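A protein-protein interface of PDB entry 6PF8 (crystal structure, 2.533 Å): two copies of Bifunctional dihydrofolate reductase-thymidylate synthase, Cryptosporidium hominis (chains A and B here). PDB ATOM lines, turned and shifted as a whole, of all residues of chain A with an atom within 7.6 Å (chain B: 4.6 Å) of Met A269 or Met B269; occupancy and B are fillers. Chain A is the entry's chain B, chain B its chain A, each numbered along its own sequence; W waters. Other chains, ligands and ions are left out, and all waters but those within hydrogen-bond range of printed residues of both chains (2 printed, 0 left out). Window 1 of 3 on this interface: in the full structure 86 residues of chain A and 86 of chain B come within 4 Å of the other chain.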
ATOM      1  N   GLN A 239     -24.595   4.208  20.491  1.00  0.00           N
ATOM      2  CA  GLN A 239     -24.073   3.496  19.331  1.00  0.00           C
ATOM      3  C   GLN A 239     -22.606   3.134  19.522  1.00  0.00           C
ATOM      4  O   GLN A 239     -22.157   2.071  19.077  1.00  0.00           O
ATOM      5  CB  GLN A 239     -24.260   4.341  18.074  1.00  0.00           C
ATOM      6  CG  GLN A 239     -25.707   4.676  17.764  1.00  0.00           C
ATOM      7  CD  GLN A 239     -26.415   3.568  17.018  1.00  0.00           C
ATOM      8  OE1 GLN A 239     -25.873   3.000  16.071  1.00  0.00           O
ATOM      9  NE2 GLN A 239     -27.636   3.258  17.438  1.00  0.00           N
ATOM     10  N   TYR A 240     -21.841   4.004  20.184  1.00  0.00           N
ATOM     11  CA  TYR A 240     -20.443   3.691  20.454  1.00  0.00           C
ATOM     12  C   TYR A 240     -20.288   2.846  21.712  1.00  0.00           C
ATOM     13  O   TYR A 240     -19.529   1.870  21.716  1.00  0.00           O
ATOM     14  CB  TYR A 240     -19.623   4.978  20.570  1.00  0.00           C
ATOM     15  CG  TYR A 240     -18.251   4.765  21.168  1.00  0.00           C
ATOM     16  CD1 TYR A 240     -17.204   4.272  20.401  1.00  0.00           C
ATOM     17  CD2 TYR A 240     -18.001   5.062  22.505  1.00  0.00           C
ATOM     18  CE1 TYR A 240     -15.947   4.073  20.949  1.00  0.00           C
ATOM     19  CE2 TYR A 240     -16.750   4.866  23.060  1.00  0.00           C
ATOM     20  CZ  TYR A 240     -15.727   4.374  22.276  1.00  0.00           C
ATOM     21  OH  TYR A 240     -14.480   4.178  22.819  1.00  0.00           O
ATOM     22  N   LEU A 243     -21.240  -0.761  21.294  1.00  0.00           N
ATOM     23  CA  LEU A 243     -20.242  -1.500  20.527  1.00  0.00           C
ATOM     24  C   LEU A 243     -19.092  -1.959  21.417  1.00  0.00           C
ATOM     25  O   LEU A 243     -18.579  -3.071  21.249  1.00  0.00           O
ATOM     26  CB  LEU A 243     -19.732  -0.647  19.364  1.00  0.00           C
ATOM     27  CG  LEU A 243     -18.598  -1.240  18.521  1.00  0.00           C
ATOM     28  CD1 LEU A 243     -18.927  -2.650  18.038  1.00  0.00           C
ATOM     29  CD2 LEU A 243     -18.291  -0.334  17.342  1.00  0.00           C
ATOM     30  N   ARG A 246     -20.465  -5.016  23.181  1.00  0.00           N
ATOM     31  CA  ARG A 246     -20.503  -6.185  22.309  1.00  0.00           C
ATOM     32  C   ARG A 246     -19.122  -6.814  22.175  1.00  0.00           C
ATOM     33  O   ARG A 246     -18.992  -8.044  22.125  1.00  0.00           O
ATOM     34  CB  ARG A 246     -21.054  -5.792  20.937  1.00  0.00           C
ATOM     35  CG  ARG A 246     -22.422  -6.374  20.621  1.00  0.00           C
ATOM     36  CD  ARG A 246     -23.405  -5.298  20.201  1.00  0.00           C
ATOM     37  NE  ARG A 246     -22.891  -4.482  19.105  1.00  0.00           N
ATOM     38  CZ  ARG A 246     -23.314  -3.251  18.830  1.00  0.00           C
ATOM     39  NH1 ARG A 246     -24.259  -2.689  19.575  1.00  0.00           N
ATOM     40  NH2 ARG A 246     -22.791  -2.579  17.814  1.00  0.00           N
ATOM     41  N   GLY A 267     -17.487  -6.952  11.644  1.00  0.00           N
ATOM     42  CA  GLY A 267     -18.733  -6.528  11.025  1.00  0.00           C
ATOM     43  C   GLY A 267     -19.698  -5.828  11.961  1.00  0.00           C
ATOM     44  O   GLY A 267     -20.612  -6.456  12.503  1.00  0.00           O
ATOM     45  N   GLN A 268     -19.513  -4.523  12.154  1.00  0.00           N
ATOM     46  CA  GLN A 268     -20.346  -3.738  13.054  1.00  0.00           C
ATOM     47  C   GLN A 268     -20.629  -2.390  12.412  1.00  0.00           C
ATOM     48  O   GLN A 268     -20.032  -2.029  11.393  1.00  0.00           O
ATOM     49  CB  GLN A 268     -19.677  -3.560  14.423  1.00  0.00           C
ATOM     50  CG  GLN A 268     -19.500  -4.852  15.204  1.00  0.00           C
ATOM     51  CD  GLN A 268     -20.805  -5.374  15.776  1.00  0.00           C
ATOM     52  OE1 GLN A 268     -21.564  -4.629  16.393  1.00  0.00           O
ATOM     53  NE2 GLN A 268     -21.070  -6.658  15.576  1.00  0.00           N
ATOM     54  N   MET A 269     -21.556  -1.641  13.007  1.00  0.00           N
ATOM     55  CA  MET A 269     -21.884  -0.324  12.481  1.00  0.00           C
ATOM     56  C   MET A 269     -22.363   0.587  13.604  1.00  0.00           C
ATOM     57  O   MET A 269     -22.798   0.129  14.663  1.00  0.00           O
ATOM     58  CB  MET A 269     -22.941  -0.399  11.370  1.00  0.00           C
ATOM     59  CG  MET A 269     -24.371  -0.516  11.853  1.00  0.00           C
ATOM     60  SD  MET A 269     -25.543  -0.062  10.553  1.00  0.00           S
ATOM     61  CE  MET A 269     -27.106  -0.451  11.332  1.00  0.00           C
ATOM     62  N   MET A 270     -22.259   1.895  13.350  1.00  0.00           N
ATOM     63  CA  MET A 270     -22.716   2.944  14.254  1.00  0.00           C
ATOM     64  C   MET A 270     -23.343   4.062  13.435  1.00  0.00           C
ATOM     65  O   MET A 270     -22.806   4.447  12.392  1.00  0.00           O
ATOM     66  CB  MET A 270     -21.565   3.527  15.095  1.00  0.00           C
ATOM     67  CG  MET A 270     -20.877   2.566  16.055  1.00  0.00           C
ATOM     68  SD  MET A 270     -19.476   3.353  16.896  1.00  0.00           S
ATOM     69  CE  MET A 270     -18.406   3.704  15.503  1.00  0.00           C
ATOM     70  N   ARG A 271     -24.471   4.588  13.909  1.00  0.00           N
ATOM     71  CA  ARG A 271     -25.121   5.739  13.293  1.00  0.00           C
ATOM     72  C   ARG A 271     -25.064   6.932  14.236  1.00  0.00           C
ATOM     73  O   ARG A 271     -25.187   6.778  15.455  1.00  0.00           O
ATOM     74  CB  ARG A 271     -26.584   5.458  12.941  1.00  0.00           C
ATOM     75  CG  ARG A 271     -26.858   4.134  12.273  1.00  0.00           C
ATOM     76  CD  ARG A 271     -28.290   4.106  11.770  1.00  0.00           C
ATOM     77  NE  ARG A 271     -28.406   4.774  10.480  1.00  0.00           N
ATOM     78  CZ  ARG A 271     -28.613   4.138   9.333  1.00  0.00           C
ATOM     79  NH1 ARG A 271     -28.747   2.819   9.321  1.00  0.00           N
ATOM     80  NH2 ARG A 271     -28.697   4.823   8.200  1.00  0.00           N
ATOM     81  N   PHE A 272     -24.908   8.122  13.667  1.00  0.00           N
ATOM     82  CA  PHE A 272     -24.907   9.354  14.443  1.00  0.00           C
ATOM     83  C   PHE A 272     -25.665  10.425  13.679  1.00  0.00           C
ATOM     84  O   PHE A 272     -25.465  10.589  12.473  1.00  0.00           O
ATOM     85  CB  PHE A 272     -23.484   9.839  14.732  1.00  0.00           C
ATOM     86  CG  PHE A 272     -22.654   8.861  15.499  1.00  0.00           C
ATOM     87  CD1 PHE A 272     -22.739   8.797  16.878  1.00  0.00           C
ATOM     88  CD2 PHE A 272     -21.773   8.015  14.844  1.00  0.00           C
ATOM     89  CE1 PHE A 272     -21.970   7.898  17.592  1.00  0.00           C
ATOM     90  CE2 PHE A 272     -21.000   7.119  15.550  1.00  0.00           C
ATOM     91  CZ  PHE A 272     -21.099   7.060  16.926  1.00  0.00           C
ATOM     92  N   LEU A 420     -18.891   5.718   5.969  1.00  0.00           N
ATOM     93  CA  LEU A 420     -17.470   5.408   6.064  1.00  0.00           C
ATOM     94  C   LEU A 420     -17.296   3.917   6.311  1.00  0.00           C
ATOM     95  O   LEU A 420     -17.971   3.350   7.174  1.00  0.00           O
ATOM     96  CB  LEU A 420     -16.809   6.205   7.192  1.00  0.00           C
ATOM     97  CG  LEU A 420     -15.395   5.747   7.551  1.00  0.00           C
ATOM     98  CD1 LEU A 420     -14.442   6.015   6.399  1.00  0.00           C
ATOM     99  CD2 LEU A 420     -14.912   6.422   8.823  1.00  0.00           C
ATOM    100  N   ALA A 457     -22.828   7.451   9.190  1.00  0.00           N
ATOM    101  CA  ALA A 457     -22.837   6.012   9.423  1.00  0.00           C
ATOM    102  C   ALA A 457     -21.428   5.468   9.235  1.00  0.00           C
ATOM    103  O   ALA A 457     -20.768   5.777   8.237  1.00  0.00           O
ATOM    104  CB  ALA A 457     -23.823   5.305   8.492  1.00  0.00           C
ATOM    105  N   ILE A 458     -20.973   4.664  10.191  1.00  0.00           N
ATOM    106  CA  ILE A 458     -19.634   4.084  10.170  1.00  0.00           C
ATOM    107  C   ILE A 458     -19.769   2.567  10.191  1.00  0.00           C
ATOM    108  O   ILE A 458     -20.321   2.002  11.142  1.00  0.00           O
ATOM    109  CB  ILE A 458     -18.780   4.577  11.348  1.00  0.00           C
ATOM    110  CG1 ILE A 458     -18.651   6.104  11.306  1.00  0.00           C
ATOM    111  CG2 ILE A 458     -17.406   3.928  11.322  1.00  0.00           C
ATOM    112  CD1 ILE A 458     -17.778   6.676  12.396  1.00  0.00           C
ATOM    113  N   PHE A 459     -19.272   1.914   9.142  1.00  0.00           N
ATOM    114  CA  PHE A 459     -19.271   0.461   9.024  1.00  0.00           C
ATOM    115  C   PHE A 459     -17.859  -0.055   9.272  1.00  0.00           C
ATOM    116  O   PHE A 459     -16.898   0.445   8.678  1.00  0.00           O
ATOM    117  CB  PHE A 459     -19.776   0.029   7.647  1.00  0.00           C
ATOM    118  CG  PHE A 459     -21.095   0.647   7.266  1.00  0.00           C
ATOM    119  CD1 PHE A 459     -22.257   0.315   7.947  1.00  0.00           C
ATOM    120  CD2 PHE A 459     -21.172   1.573   6.240  1.00  0.00           C
ATOM    121  CE1 PHE A 459     -23.472   0.881   7.600  1.00  0.00           C
ATOM    122  CE2 PHE A 459     -22.384   2.149   5.891  1.00  0.00           C
ATOM    123  CZ  PHE A 459     -23.534   1.802   6.573  1.00  0.00           C
ATOM    124  N   ILE A 460     -17.739  -1.054  10.142  1.00  0.00           N
ATOM    125  CA  ILE A 460     -16.456  -1.464  10.700  1.00  0.00           C
ATOM    126  C   ILE A 460     -16.185  -2.924  10.371  1.00  0.00           C
ATOM    127  O   ILE A 460     -17.074  -3.776  10.489  1.00  0.00           O
ATOM    128  CB  ILE A 460     -16.417  -1.245  12.226  1.00  0.00           C
ATOM    129  CG1 ILE A 460     -16.636   0.231  12.556  1.00  0.00           C
ATOM    130  CG2 ILE A 460     -15.103  -1.758  12.803  1.00  0.00           C
ATOM    131  CD1 ILE A 460     -16.691   0.521  14.034  1.00  0.00           C
ATOM    132  N   GLY A 461     -14.948  -3.209   9.971  1.00  0.00           N
ATOM    133  CA  GLY A 461     -14.491  -4.575   9.839  1.00  0.00           C
ATOM    134  C   GLY A 461     -14.044  -5.145  11.171  1.00  0.00           C
ATOM    135  O   GLY A 461     -14.862  -5.662  11.936  1.00  0.00           O
ATOM    136  N   ALA A 463     -13.408  -4.593  14.556  1.00  0.00           N
ATOM    137  CA  ALA A 463     -13.596  -3.767  15.744  1.00  0.00           C
ATOM    138  C   ALA A 463     -13.000  -4.482  16.950  1.00  0.00           C
ATOM    139  O   ALA A 463     -13.357  -5.630  17.235  1.00  0.00           O
ATOM    140  CB  ALA A 463     -15.079  -3.477  15.979  1.00  0.00           C
ATOM    141  N   GLN B 239     -33.409 -10.061   6.649  1.00  0.00           N
ATOM    142  CA  GLN B 239     -32.445  -8.983   6.467  1.00  0.00           C
ATOM    143  C   GLN B 239     -32.623  -8.303   5.117  1.00  0.00           C
ATOM    144  O   GLN B 239     -32.438  -7.085   5.007  1.00  0.00           O
ATOM    145  CB  GLN B 239     -31.024  -9.518   6.612  1.00  0.00           C
ATOM    146  CG  GLN B 239     -30.742 -10.131   7.969  1.00  0.00           C
ATOM    147  CD  GLN B 239     -30.389  -9.093   9.007  1.00  0.00           C
ATOM    148  OE1 GLN B 239     -29.599  -8.184   8.747  1.00  0.00           O
ATOM    149  NE2 GLN B 239     -30.973  -9.217  10.191  1.00  0.00           N
ATOM    150  N   ARG B 246     -38.170  -0.962   4.607  1.00  0.00           N
ATOM    151  CA  ARG B 246     -37.634   0.327   5.031  1.00  0.00           C
ATOM    152  C   ARG B 246     -37.584   1.312   3.871  1.00  0.00           C
ATOM    153  O   ARG B 246     -37.847   2.508   4.049  1.00  0.00           O
ATOM    154  CB  ARG B 246     -36.244   0.137   5.637  1.00  0.00           C
ATOM    155  CG  ARG B 246     -36.166   0.405   7.128  1.00  0.00           C
ATOM    156  CD  ARG B 246     -35.546  -0.769   7.867  1.00  0.00           C
ATOM    157  NE  ARG B 246     -34.255  -1.157   7.308  1.00  0.00           N
ATOM    158  CZ  ARG B 246     -33.720  -2.366   7.459  1.00  0.00           C
ATOM    159  NH1 ARG B 246     -34.374  -3.296   8.144  1.00  0.00           N
ATOM    160  NH2 ARG B 246     -32.540  -2.650   6.921  1.00  0.00           N
ATOM    161  N   GLN B 268     -27.347   1.422   4.989  1.00  0.00           N
ATOM    162  CA  GLN B 268     -28.068   0.250   5.473  1.00  0.00           C
ATOM    163  C   GLN B 268     -27.119  -0.940   5.518  1.00  0.00           C
ATOM    164  O   GLN B 268     -26.004  -0.890   4.992  1.00  0.00           O
ATOM    165  CB  GLN B 268     -29.286  -0.062   4.595  1.00  0.00           C
ATOM    166  CG  GLN B 268     -30.364   1.011   4.620  1.00  0.00           C
ATOM    167  CD  GLN B 268     -31.147   1.033   5.920  1.00  0.00           C
ATOM    168  OE1 GLN B 268     -31.611  -0.003   6.394  1.00  0.00           O
ATOM    169  NE2 GLN B 268     -31.290   2.216   6.509  1.00  0.00           N
ATOM    170  N   MET B 269     -27.564  -2.021   6.162  1.00  0.00           N
ATOM    171  CA  MET B 269     -26.735  -3.214   6.254  1.00  0.00           C
ATOM    172  C   MET B 269     -27.605  -4.461   6.359  1.00  0.00           C
ATOM    173  O   MET B 269     -28.770  -4.404   6.763  1.00  0.00           O
ATOM    174  CB  MET B 269     -25.768  -3.137   7.444  1.00  0.00           C
ATOM    175  CG  MET B 269     -26.377  -3.485   8.790  1.00  0.00           C
ATOM    176  SD  MET B 269     -25.103  -3.871  10.014  1.00  0.00           S
ATOM    177  CE  MET B 269     -26.097  -4.058  11.491  1.00  0.00           C
ATOM    178  N   MET B 270     -27.008  -5.595   5.987  1.00  0.00           N
ATOM    179  CA  MET B 270     -27.636  -6.909   6.050  1.00  0.00           C
ATOM    180  C   MET B 270     -26.595  -7.925   6.504  1.00  0.00           C
ATOM    181  O   MET B 270     -25.445  -7.880   6.058  1.00  0.00           O
ATOM    182  CB  MET B 270     -28.206  -7.345   4.687  1.00  0.00           C
ATOM    183  CG  MET B 270     -29.317  -6.472   4.109  1.00  0.00           C
ATOM    184  SD  MET B 270     -29.833  -7.030   2.461  1.00  0.00           S
ATOM    185  CE  MET B 270     -28.320  -6.804   1.533  1.00  0.00           C
ATOM    186  N   ARG B 271     -26.997  -8.836   7.388  1.00  0.00           N
ATOM    187  CA  ARG B 271     -26.145  -9.932   7.832  1.00  0.00           C
ATOM    188  C   ARG B 271     -26.710 -11.257   7.339  1.00  0.00           C
ATOM    189  O   ARG B 271     -27.929 -11.444   7.296  1.00  0.00           O
ATOM    190  CB  ARG B 271     -26.027  -9.978   9.359  1.00  0.00           C
ATOM    191  CG  ARG B 271     -25.791  -8.644  10.032  1.00  0.00           C
ATOM    192  CD  ARG B 271     -25.456  -8.845  11.503  1.00  0.00           C
ATOM    193  NE  ARG B 271     -24.048  -9.175  11.685  1.00  0.00           N
ATOM    194  CZ  ARG B 271     -23.148  -8.345  12.202  1.00  0.00           C
ATOM    195  NH1 ARG B 271     -23.509  -7.136  12.606  1.00  0.00           N
ATOM    196  NH2 ARG B 271     -21.885  -8.731  12.322  1.00  0.00           N
ATOM    197  N   ILE B 458     -23.177  -7.036   4.472  1.00  0.00           N
ATOM    198  CA  ILE B 458     -23.205  -6.140   3.321  1.00  0.00           C
ATOM    199  C   ILE B 458     -23.621  -4.759   3.807  1.00  0.00           C
ATOM    200  O   ILE B 458     -24.729  -4.587   4.329  1.00  0.00           O
ATOM    201  CB  ILE B 458     -24.157  -6.646   2.226  1.00  0.00           C
ATOM    202  CG1 ILE B 458     -23.726  -8.036   1.749  1.00  0.00           C
ATOM    203  CG2 ILE B 458     -24.204  -5.664   1.066  1.00  0.00           C
ATOM    204  CD1 ILE B 458     -24.577  -8.586   0.629  1.00  0.00           C
ATOM    205  N   PHE B 459     -22.739  -3.779   3.630  1.00  0.00           N
ATOM    206  CA  PHE B 459     -23.006  -2.395   4.002  1.00  0.00           C
ATOM    207  C   PHE B 459     -23.294  -1.593   2.740  1.00  0.00           C
ATOM    208  O   PHE B 459     -22.540  -1.672   1.765  1.00  0.00           O
ATOM    209  CB  PHE B 459     -21.824  -1.801   4.769  1.00  0.00           C
ATOM    210  CG  PHE B 459     -21.365  -2.647   5.924  1.00  0.00           C
ATOM    211  CD1 PHE B 459     -22.178  -2.832   7.033  1.00  0.00           C
ATOM    212  CD2 PHE B 459     -20.126  -3.263   5.901  1.00  0.00           C
ATOM    213  CE1 PHE B 459     -21.758  -3.608   8.101  1.00  0.00           C
ATOM    214  CE2 PHE B 459     -19.700  -4.044   6.964  1.00  0.00           C
ATOM    215  CZ  PHE B 459     -20.519  -4.216   8.065  1.00  0.00           C
HETATM  216  O   HOH W   1     -30.831   4.879   6.059  1.00  0.00           O
HETATM  217  O   HOH W   2     -19.784  -8.814  14.512  1.00  0.00           O
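Among the printed residues, pairs that only touch across the chains: Gln A268 with Arg B271, Met A269 with Met B269, Arg A271 with Gln B268, Phe A459 with Gln B268 and Phe A459 with Phe B459.
Printed residues of chain B that touch a printed residue of chain A: Gln B268, Met B269, Arg B271 and Phe B459. Along chain B the printed residues that touch a printed residue of chain A span positions 268 to 459. Among the printed residues, 6 pairs touch across the chains. Among the printed residues, no Asp or Glu carboxylate lies within 4 Å of a Lys or Arg side-chain nitrogen of the other chain.
NH2 of Arg B271 is in hydrogen-bond range of O of Gly A267 (2.6 Å).
Tyr A240 touches none of the printed residues of chain B. Of the printed residues of chain B, Gln A268 touches Arg B271. Met A270 touches none of the printed residues of chain B. Of the printed residues of chain B, Phe A459 touches Gln B268 (3.98 Å) and Phe B459 (3.3 Å). Printed residues of chain A within 4 Å of Gln B268: Arg A271 and Phe A459. Of chain A, only Met A269 (3.7 Å) comes within 4 Å of Met B269. The nearest printed residue of chain B that does not touch Met A269 is Phe B459 (4.7 Å). The nearest printed residue of chain A that does not touch Phe B459 is Gln A268 (4.01 Å).
Water W2 lies within hydrogen-bond range of NE2 of Gln A268, NH2 of Arg B271 and O of Gly A267. Water W1 bridges the side-chain amide nitrogen (NE2) of Gln B268 (2.7 Å) and the guanidinium group (NH2) of Arg A271 (3.0 Å).
Gln A268 touches Arg B271, and with the chains exchanged Arg A271 touches Gln B268. Met B269 touches its own counterpart, Met A269. Phe A459 touches Gln B268, but with the chains exchanged Gln A268 does not touch Phe B459 (4.01 Å). Phe A459 touches its own counterpart, Phe B459. Positions printed for both chains: 239, 246, 268, 269, 270, 271, 458 and 459.
The side-chain amide oxygen (OE1) of Gln B239 is in hydrogen-bond range of the backbone NH (N) of Arg B271, 3.0 Å away. NH2 of Arg B246 sits at hydrogen-bond distance from OE1 of Gln B268. The backbone NH of Arg A271 sits at hydrogen-bond distance from the side-chain amide oxygen of Gln A239 (3.0 Å). The side-chain amide oxygen (OE1) of Gln A268 is in hydrogen-bond range of the guanidinium group (NH2) of Arg A246 (2.8 Å). The backbone carbonyl oxygen (O) of Gly A461 is in hydrogen-bond range of the backbone NH (N) of Gly A267 (2.9 Å). The backbone carbonyl oxygen of Leu A420 lies within hydrogen-bond range of the backbone NH of Phe A459 (2.8 Å).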
